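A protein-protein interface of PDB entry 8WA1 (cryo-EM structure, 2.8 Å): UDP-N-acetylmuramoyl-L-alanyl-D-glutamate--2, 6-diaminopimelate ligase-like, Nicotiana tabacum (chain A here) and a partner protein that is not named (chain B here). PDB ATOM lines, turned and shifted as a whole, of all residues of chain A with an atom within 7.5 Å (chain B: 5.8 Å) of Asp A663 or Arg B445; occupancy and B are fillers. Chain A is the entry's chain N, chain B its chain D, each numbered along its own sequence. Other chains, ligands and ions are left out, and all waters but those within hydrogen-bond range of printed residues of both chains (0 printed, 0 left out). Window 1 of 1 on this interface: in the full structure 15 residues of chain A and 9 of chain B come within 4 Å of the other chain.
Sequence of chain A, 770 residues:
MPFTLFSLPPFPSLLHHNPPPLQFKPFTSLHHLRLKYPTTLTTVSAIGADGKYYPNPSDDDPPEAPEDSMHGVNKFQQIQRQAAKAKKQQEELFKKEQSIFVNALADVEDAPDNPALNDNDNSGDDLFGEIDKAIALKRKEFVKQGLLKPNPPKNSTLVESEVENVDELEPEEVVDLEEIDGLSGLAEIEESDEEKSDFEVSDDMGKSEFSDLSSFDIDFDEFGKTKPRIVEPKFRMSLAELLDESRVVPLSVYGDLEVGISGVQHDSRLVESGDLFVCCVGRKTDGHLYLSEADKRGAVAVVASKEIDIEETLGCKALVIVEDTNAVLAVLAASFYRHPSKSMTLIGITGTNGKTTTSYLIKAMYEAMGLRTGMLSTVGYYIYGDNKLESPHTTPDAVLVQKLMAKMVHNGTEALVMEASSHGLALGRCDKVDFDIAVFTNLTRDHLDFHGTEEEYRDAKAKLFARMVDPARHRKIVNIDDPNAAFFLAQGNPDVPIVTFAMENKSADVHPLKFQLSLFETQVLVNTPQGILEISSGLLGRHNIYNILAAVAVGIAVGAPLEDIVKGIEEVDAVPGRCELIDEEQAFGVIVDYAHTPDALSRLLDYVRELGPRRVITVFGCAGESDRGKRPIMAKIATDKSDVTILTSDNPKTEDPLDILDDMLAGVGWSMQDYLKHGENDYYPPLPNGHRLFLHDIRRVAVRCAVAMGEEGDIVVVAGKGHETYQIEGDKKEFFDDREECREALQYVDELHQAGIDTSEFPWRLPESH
O of Arg A628 is in hydrogen-bond range of OH of Tyr B435, 3.0 Å away. O of Asp A659 is in hydrogen-bond range of NH1 of Arg B447. The guanidinium group of Arg B445 lies within salt-bridge range of the side-chain carboxylate of Asp A662 (3.6 Å). The side-chain carboxylate (OD2) of Asp A662 lies within hydrogen-bond range of the backbone NH (N) of Trp B448, at 3.1 Å. OD2 of Asp A663 lies within hydrogen-bond range of OH of Tyr B435 (3.4 Å). The side-chain carboxylate (OD1) of Asp A663 is in salt-bridge range of the guanidinium group (NH2) of Arg B445 (3.5 Å). The backbone carbonyl oxygen (O) of Trp B448 is in hydrogen-bond range of the backbone NH (N) of Met A672 (3.4 Å).
The side-chain carboxylate (OD1) of Asp A627 lies within hydrogen-bond range of the backbone NH (N) of Gly A629, 3.2 Å away. The side-chain carboxylate (OD1) of Asp A662 sits at hydrogen-bond distance from the backbone NH (N) of Met A672 (2.8 Å). The guanidinium group (NE) of Arg B445 lies within salt-bridge range of the side-chain carboxylate (OE2) of Glu B438, 2.8 Å away.
Among the printed residues, merely in contact across the chains: Gly A629 with Tyr B435 (3.8 Å), Pro A632 with Tyr B435 (3.4 Å), Asp A662 with Arg B447 (3.1 Å), Ala A666 with Arg B445 (3.5 Å) and Ser A671 with Trp B448 (3.7 Å).
Of the printed residues of chain B, Asp A659 touches Arg B447. Ile A660 touches none of the printed residues of chain B. Leu A661 touches none of the printed residues of chain B. Of chain B, only Tyr B435 (3.1 Å) and Arg B445 (3.5 Å) come within 4 Å of Asp A663. Printed residues of chain A within 4 Å of Trp B448: Asp A662, Ser A671 and Met A672. The nearest residue of chain A that does not touch Arg B445 is Asp A659 (5.6 Å).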
ATOM      1  N   ASP A 627     -21.595  -5.441  26.313  1.00  0.00           N
ATOM      2  CA  ASP A 627     -22.981  -5.850  26.270  1.00  0.00           C
ATOM      3  C   ASP A 627     -23.335  -5.912  24.804  1.00  0.00           C
ATOM      4  O   ASP A 627     -23.076  -4.971  24.053  1.00  0.00           O
ATOM      5  CB  ASP A 627     -23.864  -4.822  26.965  1.00  0.00           C
ATOM      6  CG  ASP A 627     -25.340  -5.095  26.771  1.00  0.00           C
ATOM      7  OD1 ASP A 627     -25.757  -6.258  26.938  1.00  0.00           O
ATOM      8  OD2 ASP A 627     -26.086  -4.147  26.451  1.00  0.00           O
ATOM      9  N   ARG A 628     -23.941  -7.012  24.387  1.00  0.00           N
ATOM     10  CA  ARG A 628     -24.272  -7.161  22.986  1.00  0.00           C
ATOM     11  C   ARG A 628     -25.660  -6.619  22.753  1.00  0.00           C
ATOM     12  O   ARG A 628     -26.108  -6.526  21.619  1.00  0.00           O
ATOM     13  CB  ARG A 628     -24.150  -8.622  22.563  1.00  0.00           C
ATOM     14  N   GLY A 629     -26.342  -6.246  23.826  1.00  0.00           N
ATOM     15  CA  GLY A 629     -27.661  -5.665  23.700  1.00  0.00           C
ATOM     16  C   GLY A 629     -27.524  -4.373  22.935  1.00  0.00           C
ATOM     17  O   GLY A 629     -28.391  -4.014  22.143  1.00  0.00           O
ATOM     18  N   LYS A 630     -26.439  -3.656  23.182  1.00  0.00           N
ATOM     19  CA  LYS A 630     -26.203  -2.398  22.499  1.00  0.00           C
ATOM     20  C   LYS A 630     -26.071  -2.574  21.010  1.00  0.00           C
ATOM     21  O   LYS A 630     -26.462  -1.699  20.248  1.00  0.00           O
ATOM     22  CB  LYS A 630     -24.905  -1.783  22.996  1.00  0.00           C
ATOM     23  CG  LYS A 630     -24.783  -1.660  24.500  1.00  0.00           C
ATOM     24  CD  LYS A 630     -23.319  -1.551  24.882  1.00  0.00           C
ATOM     25  CE  LYS A 630     -22.570  -0.674  23.891  1.00  0.00           C
ATOM     26  NZ  LYS A 630     -21.101  -0.692  24.126  1.00  0.00           N
ATOM     27  N   ARG A 631     -25.522  -3.694  20.570  1.00  0.00           N
ATOM     28  CA  ARG A 631     -25.227  -3.833  19.147  1.00  0.00           C
ATOM     29  C   ARG A 631     -26.348  -3.717  18.127  1.00  0.00           C
ATOM     30  O   ARG A 631     -26.185  -3.030  17.122  1.00  0.00           O
ATOM     31  CB  ARG A 631     -24.462  -5.144  18.910  1.00  0.00           C
ATOM     32  N   PRO A 632     -27.491  -4.368  18.358  1.00  0.00           N
ATOM     33  CA  PRO A 632     -28.490  -4.182  17.305  1.00  0.00           C
ATOM     34  C   PRO A 632     -28.978  -2.753  17.182  1.00  0.00           C
ATOM     35  O   PRO A 632     -29.093  -2.254  16.065  1.00  0.00           O
ATOM     36  CB  PRO A 632     -29.637  -5.088  17.746  1.00  0.00           C
ATOM     37  CG  PRO A 632     -29.405  -5.331  19.195  1.00  0.00           C
ATOM     38  CD  PRO A 632     -27.920  -5.398  19.313  1.00  0.00           C
ATOM     39  N   ILE A 633     -29.252  -2.091  18.300  1.00  0.00           N
ATOM     40  CA  ILE A 633     -29.820  -0.746  18.239  1.00  0.00           C
ATOM     41  C   ILE A 633     -28.903   0.286  17.613  1.00  0.00           C
ATOM     42  O   ILE A 633     -29.334   1.069  16.776  1.00  0.00           O
ATOM     43  CB  ILE A 633     -30.329  -0.289  19.627  1.00  0.00           C
ATOM     44  CG1 ILE A 633     -30.390   1.237  19.721  1.00  0.00           C
ATOM     45  CG2 ILE A 633     -29.470  -0.857  20.742  1.00  0.00           C
ATOM     46  CD1 ILE A 633     -30.795   1.748  21.083  1.00  0.00           C
ATOM     47  N   ALA A 635     -26.456   0.107  15.360  1.00  0.00           N
ATOM     48  CA  ALA A 635     -26.427   0.021  13.904  1.00  0.00           C
ATOM     49  C   ALA A 635     -27.680   0.638  13.294  1.00  0.00           C
ATOM     50  O   ALA A 635     -27.599   1.373  12.303  1.00  0.00           O
ATOM     51  CB  ALA A 635     -26.272  -1.433  13.465  1.00  0.00           C
ATOM     52  N   PRO A 657     -14.019 -10.791  14.574  1.00  0.00           N
ATOM     53  CA  PRO A 657     -14.595  -9.540  14.047  1.00  0.00           C
ATOM     54  C   PRO A 657     -15.892  -9.753  13.287  1.00  0.00           C
ATOM     55  O   PRO A 657     -16.853  -9.000  13.486  1.00  0.00           O
ATOM     56  CB  PRO A 657     -13.483  -8.999  13.136  1.00  0.00           C
ATOM     57  CG  PRO A 657     -12.232  -9.670  13.612  1.00  0.00           C
ATOM     58  CD  PRO A 657     -12.656 -11.029  14.071  1.00  0.00           C
ATOM     59  N   LEU A 658     -15.950 -10.766  12.419  1.00  0.00           N
ATOM     60  CA  LEU A 658     -17.170 -11.020  11.660  1.00  0.00           C
ATOM     61  C   LEU A 658     -18.291 -11.521  12.563  1.00  0.00           C
ATOM     62  O   LEU A 658     -19.473 -11.397  12.219  1.00  0.00           O
ATOM     63  CB  LEU A 658     -16.898 -12.023  10.537  1.00  0.00           C
ATOM     64  CG  LEU A 658     -16.189 -11.525   9.271  1.00  0.00           C
ATOM     65  CD1 LEU A 658     -14.694 -11.336   9.494  1.00  0.00           C
ATOM     66  CD2 LEU A 658     -16.445 -12.475   8.110  1.00  0.00           C
ATOM     67  N   ASP A 659     -17.943 -12.102  13.713  1.00  0.00           N
ATOM     68  CA  ASP A 659     -18.960 -12.616  14.626  1.00  0.00           C
ATOM     69  C   ASP A 659     -19.786 -11.506  15.265  1.00  0.00           C
ATOM     70  O   ASP A 659     -20.984 -11.698  15.496  1.00  0.00           O
ATOM     71  CB  ASP A 659     -18.306 -13.467  15.715  1.00  0.00           C
ATOM     72  N   ILE A 660     -19.179 -10.354  15.553  1.00  0.00           N
ATOM     73  CA  ILE A 660     -19.925  -9.261  16.167  1.00  0.00           C
ATOM     74  C   ILE A 660     -20.561  -8.379  15.099  1.00  0.00           C
ATOM     75  O   ILE A 660     -21.599  -7.749  15.335  1.00  0.00           O
ATOM     76  CB  ILE A 660     -19.007  -8.456  17.107  1.00  0.00           C
ATOM     77  CG1 ILE A 660     -19.808  -7.407  17.882  1.00  0.00           C
ATOM     78  CG2 ILE A 660     -17.874  -7.803  16.330  1.00  0.00           C
ATOM     79  CD1 ILE A 660     -20.867  -7.996  18.791  1.00  0.00           C
ATOM     80  N   LEU A 661     -19.961  -8.327  13.906  1.00  0.00           N
ATOM     81  CA  LEU A 661     -20.553  -7.550  12.823  1.00  0.00           C
ATOM     82  C   LEU A 661     -21.881  -8.148  12.378  1.00  0.00           C
ATOM     83  O   LEU A 661     -22.794  -7.417  11.979  1.00  0.00           O
ATOM     84  CB  LEU A 661     -19.578  -7.456  11.648  1.00  0.00           C
ATOM     85  CG  LEU A 661     -18.305  -6.645  11.899  1.00  0.00           C
ATOM     86  CD1 LEU A 661     -17.404  -6.656  10.673  1.00  0.00           C
ATOM     87  CD2 LEU A 661     -18.639  -5.220  12.314  1.00  0.00           C
ATOM     88  N   ASP A 662     -22.014  -9.476  12.449  1.00  0.00           N
ATOM     89  CA  ASP A 662     -23.293 -10.103  12.131  1.00  0.00           C
ATOM     90  C   ASP A 662     -24.357  -9.727  13.154  1.00  0.00           C
ATOM     91  O   ASP A 662     -25.502  -9.432  12.792  1.00  0.00           O
ATOM     92  CB  ASP A 662     -23.135 -11.620  12.057  1.00  0.00           C
ATOM     93  CG  ASP A 662     -24.423 -12.320  11.669  1.00  0.00           C
ATOM     94  OD1 ASP A 662     -24.881 -12.131  10.522  1.00  0.00           O
ATOM     95  OD2 ASP A 662     -24.978 -13.057  12.511  1.00  0.00           O
ATOM     96  N   ASP A 663     -23.997  -9.731  14.440  1.00  0.00           N
ATOM     97  CA  ASP A 663     -24.939  -9.307  15.469  1.00  0.00           C
ATOM     98  C   ASP A 663     -25.309  -7.838  15.299  1.00  0.00           C
ATOM     99  O   ASP A 663     -26.439  -7.435  15.599  1.00  0.00           O
ATOM    100  CB  ASP A 663     -24.345  -9.556  16.856  1.00  0.00           C
ATOM    101  CG  ASP A 663     -25.385  -9.485  17.956  1.00  0.00           C
ATOM    102  OD1 ASP A 663     -26.591  -9.509  17.638  1.00  0.00           O
ATOM    103  OD2 ASP A 663     -24.994  -9.404  19.140  1.00  0.00           O
ATOM    104  N   MET A 664     -24.365  -7.023  14.821  1.00  0.00           N
ATOM    105  CA  MET A 664     -24.659  -5.616  14.573  1.00  0.00           C
ATOM    106  C   MET A 664     -25.621  -5.452  13.402  1.00  0.00           C
ATOM    107  O   MET A 664     -26.594  -4.693  13.489  1.00  0.00           O
ATOM    108  CB  MET A 664     -23.360  -4.849  14.319  1.00  0.00           C
ATOM    109  CG  MET A 664     -23.254  -3.533  15.071  1.00  0.00           C
ATOM    110  SD  MET A 664     -21.651  -2.735  14.856  1.00  0.00           S
ATOM    111  CE  MET A 664     -20.547  -4.028  15.419  1.00  0.00           C
ATOM    112  N   LEU A 665     -25.372  -6.160  12.300  1.00  0.00           N
ATOM    113  CA  LEU A 665     -26.249  -6.102  11.137  1.00  0.00           C
ATOM    114  C   LEU A 665     -27.601  -6.758  11.381  1.00  0.00           C
ATOM    115  O   LEU A 665     -28.543  -6.494  10.628  1.00  0.00           O
ATOM    116  CB  LEU A 665     -25.576  -6.766   9.933  1.00  0.00           C
ATOM    117  CG  LEU A 665     -24.290  -6.123   9.410  1.00  0.00           C
ATOM    118  CD1 LEU A 665     -23.833  -6.802   8.128  1.00  0.00           C
ATOM    119  CD2 LEU A 665     -24.489  -4.633   9.190  1.00  0.00           C
ATOM    120  N   ALA A 666     -27.714  -7.608  12.405  1.00  0.00           N
ATOM    121  CA  ALA A 666     -29.011  -8.181  12.748  1.00  0.00           C
ATOM    122  C   ALA A 666     -30.012  -7.105  13.146  1.00  0.00           C
ATOM    123  O   ALA A 666     -31.226  -7.318  13.048  1.00  0.00           O
ATOM    124  CB  ALA A 666     -28.852  -9.207  13.872  1.00  0.00           C
ATOM    125  N   GLY A 667     -29.527  -5.950  13.606  1.00  0.00           N
ATOM    126  CA  GLY A 667     -30.431  -4.871  13.972  1.00  0.00           C
ATOM    127  C   GLY A 667     -31.158  -4.281  12.778  1.00  0.00           C
ATOM    128  O   GLY A 667     -32.322  -3.888  12.881  1.00  0.00           O
ATOM    129  N   VAL A 668     -30.478  -4.200  11.627  1.00  0.00           N
ATOM    130  CA  VAL A 668     -31.095  -3.650  10.423  1.00  0.00           C
ATOM    131  C   VAL A 668     -31.774  -4.713   9.573  1.00  0.00           C
ATOM    132  O   VAL A 668     -32.413  -4.372   8.567  1.00  0.00           O
ATOM    133  CB  VAL A 668     -30.062  -2.891   9.564  1.00  0.00           C
ATOM    134  CG1 VAL A 668     -29.300  -1.884  10.414  1.00  0.00           C
ATOM    135  CG2 VAL A 668     -29.112  -3.864   8.887  1.00  0.00           C
ATOM    136  N   TRP A 670     -30.164  -7.502   8.172  1.00  0.00           N
ATOM    137  CA  TRP A 670     -29.248  -8.232   7.309  1.00  0.00           C
ATOM    138  C   TRP A 670     -28.393  -9.206   8.114  1.00  0.00           C
ATOM    139  O   TRP A 670     -28.258  -9.099   9.335  1.00  0.00           O
ATOM    140  CB  TRP A 670     -28.344  -7.271   6.538  1.00  0.00           C
ATOM    141  CG  TRP A 670     -29.040  -6.522   5.446  1.00  0.00           C
ATOM    142  CD1 TRP A 670     -30.350  -6.629   5.079  1.00  0.00           C
ATOM    143  CD2 TRP A 670     -28.458  -5.548   4.572  1.00  0.00           C
ATOM    144  NE1 TRP A 670     -30.619  -5.781   4.033  1.00  0.00           N
ATOM    145  CE2 TRP A 670     -29.474  -5.106   3.702  1.00  0.00           C
ATOM    146  CE3 TRP A 670     -27.175  -5.006   4.441  1.00  0.00           C
ATOM    147  CZ2 TRP A 670     -29.248  -4.148   2.718  1.00  0.00           C
ATOM    148  CZ3 TRP A 670     -26.953  -4.056   3.464  1.00  0.00           C
ATOM    149  CH2 TRP A 670     -27.983  -3.636   2.616  1.00  0.00           C
ATOM    150  N   SER A 671     -27.816 -10.170   7.402  1.00  0.00           N
ATOM    151  CA  SER A 671     -26.884 -11.133   7.964  1.00  0.00           C
ATOM    152  C   SER A 671     -25.579 -11.092   7.178  1.00  0.00           C
ATOM    153  O   SER A 671     -25.513 -10.540   6.074  1.00  0.00           O
ATOM    154  CB  SER A 671     -27.468 -12.552   7.945  1.00  0.00           C
ATOM    155  OG  SER A 671     -27.819 -12.937   6.627  1.00  0.00           O
ATOM    156  N   MET A 672     -24.532 -11.679   7.761  1.00  0.00           N
ATOM    157  CA  MET A 672     -23.236 -11.692   7.088  1.00  0.00           C
ATOM    158  C   MET A 672     -23.276 -12.500   5.799  1.00  0.00           C
ATOM    159  O   MET A 672     -22.598 -12.149   4.827  1.00  0.00           O
ATOM    160  CB  MET A 672     -22.156 -12.236   8.023  1.00  0.00           C
ATOM    161  CG  MET A 672     -21.518 -11.175   8.905  1.00  0.00           C
ATOM    162  SD  MET A 672     -19.762 -10.941   8.569  1.00  0.00           S
ATOM    163  CE  MET A 672     -19.788 -10.566   6.817  1.00  0.00           C
ATOM    164  N   TYR B 435     -34.104  -9.806  18.475  1.00  0.00           N
ATOM    165  CA  TYR B 435     -32.777 -10.102  18.966  1.00  0.00           C
ATOM    166  C   TYR B 435     -32.840 -10.490  20.418  1.00  0.00           C
ATOM    167  O   TYR B 435     -32.170 -11.418  20.849  1.00  0.00           O
ATOM    168  CB  TYR B 435     -31.840  -8.911  18.776  1.00  0.00           C
ATOM    169  CG  TYR B 435     -30.581  -9.024  19.587  1.00  0.00           C
ATOM    170  CD1 TYR B 435     -29.606  -9.944  19.253  1.00  0.00           C
ATOM    171  CD2 TYR B 435     -30.375  -8.224  20.699  1.00  0.00           C
ATOM    172  CE1 TYR B 435     -28.461 -10.062  20.003  1.00  0.00           C
ATOM    173  CE2 TYR B 435     -29.224  -8.329  21.445  1.00  0.00           C
ATOM    174  CZ  TYR B 435     -28.272  -9.252  21.086  1.00  0.00           C
ATOM    175  OH  TYR B 435     -27.126  -9.379  21.818  1.00  0.00           O
ATOM    176  N   GLU B 438     -34.645 -14.125  20.750  1.00  0.00           N
ATOM    177  CA  GLU B 438     -33.839 -15.318  20.522  1.00  0.00           C
ATOM    178  C   GLU B 438     -32.916 -15.471  21.704  1.00  0.00           C
ATOM    179  O   GLU B 438     -32.645 -16.581  22.155  1.00  0.00           O
ATOM    180  CB  GLU B 438     -33.071 -15.251  19.201  1.00  0.00           C
ATOM    181  CG  GLU B 438     -32.174 -14.040  19.040  1.00  0.00           C
ATOM    182  CD  GLU B 438     -31.359 -14.080  17.770  1.00  0.00           C
ATOM    183  OE1 GLU B 438     -31.170 -15.182  17.219  1.00  0.00           O
ATOM    184  OE2 GLU B 438     -30.898 -13.008  17.329  1.00  0.00           O
ATOM    185  N   GLY B 439     -32.430 -14.352  22.212  1.00  0.00           N
ATOM    186  CA  GLY B 439     -31.534 -14.368  23.346  1.00  0.00           C
ATOM    187  C   GLY B 439     -30.683 -13.173  23.044  1.00  0.00           C
ATOM    188  O   GLY B 439     -29.998 -13.135  22.024  1.00  0.00           O
ATOM    189  N   GLY B 443     -25.429 -14.358  24.868  1.00  0.00           N
ATOM    190  CA  GLY B 443     -24.518 -15.150  24.059  1.00  0.00           C
ATOM    191  C   GLY B 443     -25.060 -16.446  23.483  1.00  0.00           C
ATOM    192  O   GLY B 443     -24.349 -17.447  23.450  1.00  0.00           O
ATOM    193  N   ASP B 444     -26.311 -16.430  23.038  1.00  0.00           N
ATOM    194  CA  ASP B 444     -26.926 -17.638  22.511  1.00  0.00           C
ATOM    195  C   ASP B 444     -27.824 -17.300  21.343  1.00  0.00           C
ATOM    196  O   ASP B 444     -29.046 -17.303  21.464  1.00  0.00           O
ATOM    197  CB  ASP B 444     -27.723 -18.344  23.604  1.00  0.00           C
ATOM    198  CG  ASP B 444     -28.102 -19.761  23.226  1.00  0.00           C
ATOM    199  OD1 ASP B 444     -27.485 -20.317  22.295  1.00  0.00           O
ATOM    200  OD2 ASP B 444     -29.017 -20.319  23.866  1.00  0.00           O
ATOM    201  N   ARG B 445     -27.220 -16.991  20.210  1.00  0.00           N
ATOM    202  CA  ARG B 445     -28.003 -16.701  19.025  1.00  0.00           C
ATOM    203  C   ARG B 445     -27.333 -17.358  17.830  1.00  0.00           C
ATOM    204  O   ARG B 445     -26.138 -17.647  17.861  1.00  0.00           O
ATOM    205  CB  ARG B 445     -28.152 -15.194  18.821  1.00  0.00           C
ATOM    206  CG  ARG B 445     -26.845 -14.439  18.661  1.00  0.00           C
ATOM    207  CD  ARG B 445     -27.110 -12.973  18.373  1.00  0.00           C
ATOM    208  NE  ARG B 445     -28.085 -12.810  17.300  1.00  0.00           N
ATOM    209  CZ  ARG B 445     -27.779 -12.559  16.032  1.00  0.00           C
ATOM    210  NH1 ARG B 445     -28.744 -12.436  15.134  1.00  0.00           N
ATOM    211  NH2 ARG B 445     -26.516 -12.421  15.663  1.00  0.00           N
ATOM    212  N   LYS B 446     -28.098 -17.604  16.779  1.00  0.00           N
ATOM    213  CA  LYS B 446     -27.515 -18.193  15.602  1.00  0.00           C
ATOM    214  C   LYS B 446     -27.024 -17.073  14.730  1.00  0.00           C
ATOM    215  O   LYS B 446     -27.812 -16.325  14.164  1.00  0.00           O
ATOM    216  CB  LYS B 446     -28.556 -19.012  14.850  1.00  0.00           C
ATOM    217  CG  LYS B 446     -28.085 -20.398  14.433  1.00  0.00           C
ATOM    218  CD  LYS B 446     -26.966 -20.336  13.407  1.00  0.00           C
ATOM    219  CE  LYS B 446     -27.441 -19.706  12.108  1.00  0.00           C
ATOM    220  NZ  LYS B 446     -26.333 -19.566  11.124  1.00  0.00           N
ATOM    221  N   ARG B 447     -25.713 -16.970  14.600  1.00  0.00           N
ATOM    222  CA  ARG B 447     -25.144 -15.919  13.797  1.00  0.00           C
ATOM    223  C   ARG B 447     -24.893 -16.443  12.405  1.00  0.00           C
ATOM    224  O   ARG B 447     -24.114 -17.369  12.227  1.00  0.00           O
ATOM    225  CB  ARG B 447     -23.847 -15.446  14.424  1.00  0.00           C
ATOM    226  CG  ARG B 447     -24.033 -14.699  15.729  1.00  0.00           C
ATOM    227  CD  ARG B 447     -23.381 -15.429  16.888  1.00  0.00           C
ATOM    228  NE  ARG B 447     -23.434 -14.643  18.116  1.00  0.00           N
ATOM    229  CZ  ARG B 447     -22.490 -13.791  18.499  1.00  0.00           C
ATOM    230  NH1 ARG B 447     -21.408 -13.613  17.754  1.00  0.00           N
ATOM    231  NH2 ARG B 447     -22.626 -13.117  19.631  1.00  0.00           N
ATOM    232  N   TRP B 448     -25.546 -15.862  11.413  1.00  0.00           N
ATOM    233  CA  TRP B 448     -25.408 -16.354  10.058  1.00  0.00           C
ATOM    234  C   TRP B 448     -24.135 -15.878   9.394  1.00  0.00           C
ATOM    235  O   TRP B 448     -24.164 -14.947   8.594  1.00  0.00           O
ATOM    236  CB  TRP B 448     -26.630 -15.956   9.239  1.00  0.00           C
ATOM    237  CG  TRP B 448     -27.908 -16.543   9.766  1.00  0.00           C
ATOM    238  CD1 TRP B 448     -28.557 -16.204  10.918  1.00  0.00           C
ATOM    239  CD2 TRP B 448     -28.690 -17.574   9.156  1.00  0.00           C
ATOM    240  NE1 TRP B 448     -29.689 -16.962  11.065  1.00  0.00           N
ATOM    241  CE2 TRP B 448     -29.796 -17.809   9.995  1.00  0.00           C
ATOM    242  CE3 TRP B 448     -28.564 -18.319   7.983  1.00  0.00           C
ATOM    243  CZ2 TRP B 448     -30.766 -18.759   9.698  1.00  0.00           C
ATOM    244  CZ3 TRP B 448     -29.528 -19.260   7.689  1.00  0.00           C
ATOM    245  CH2 TRP B 448     -30.615 -19.471   8.542  1.00  0.00           C
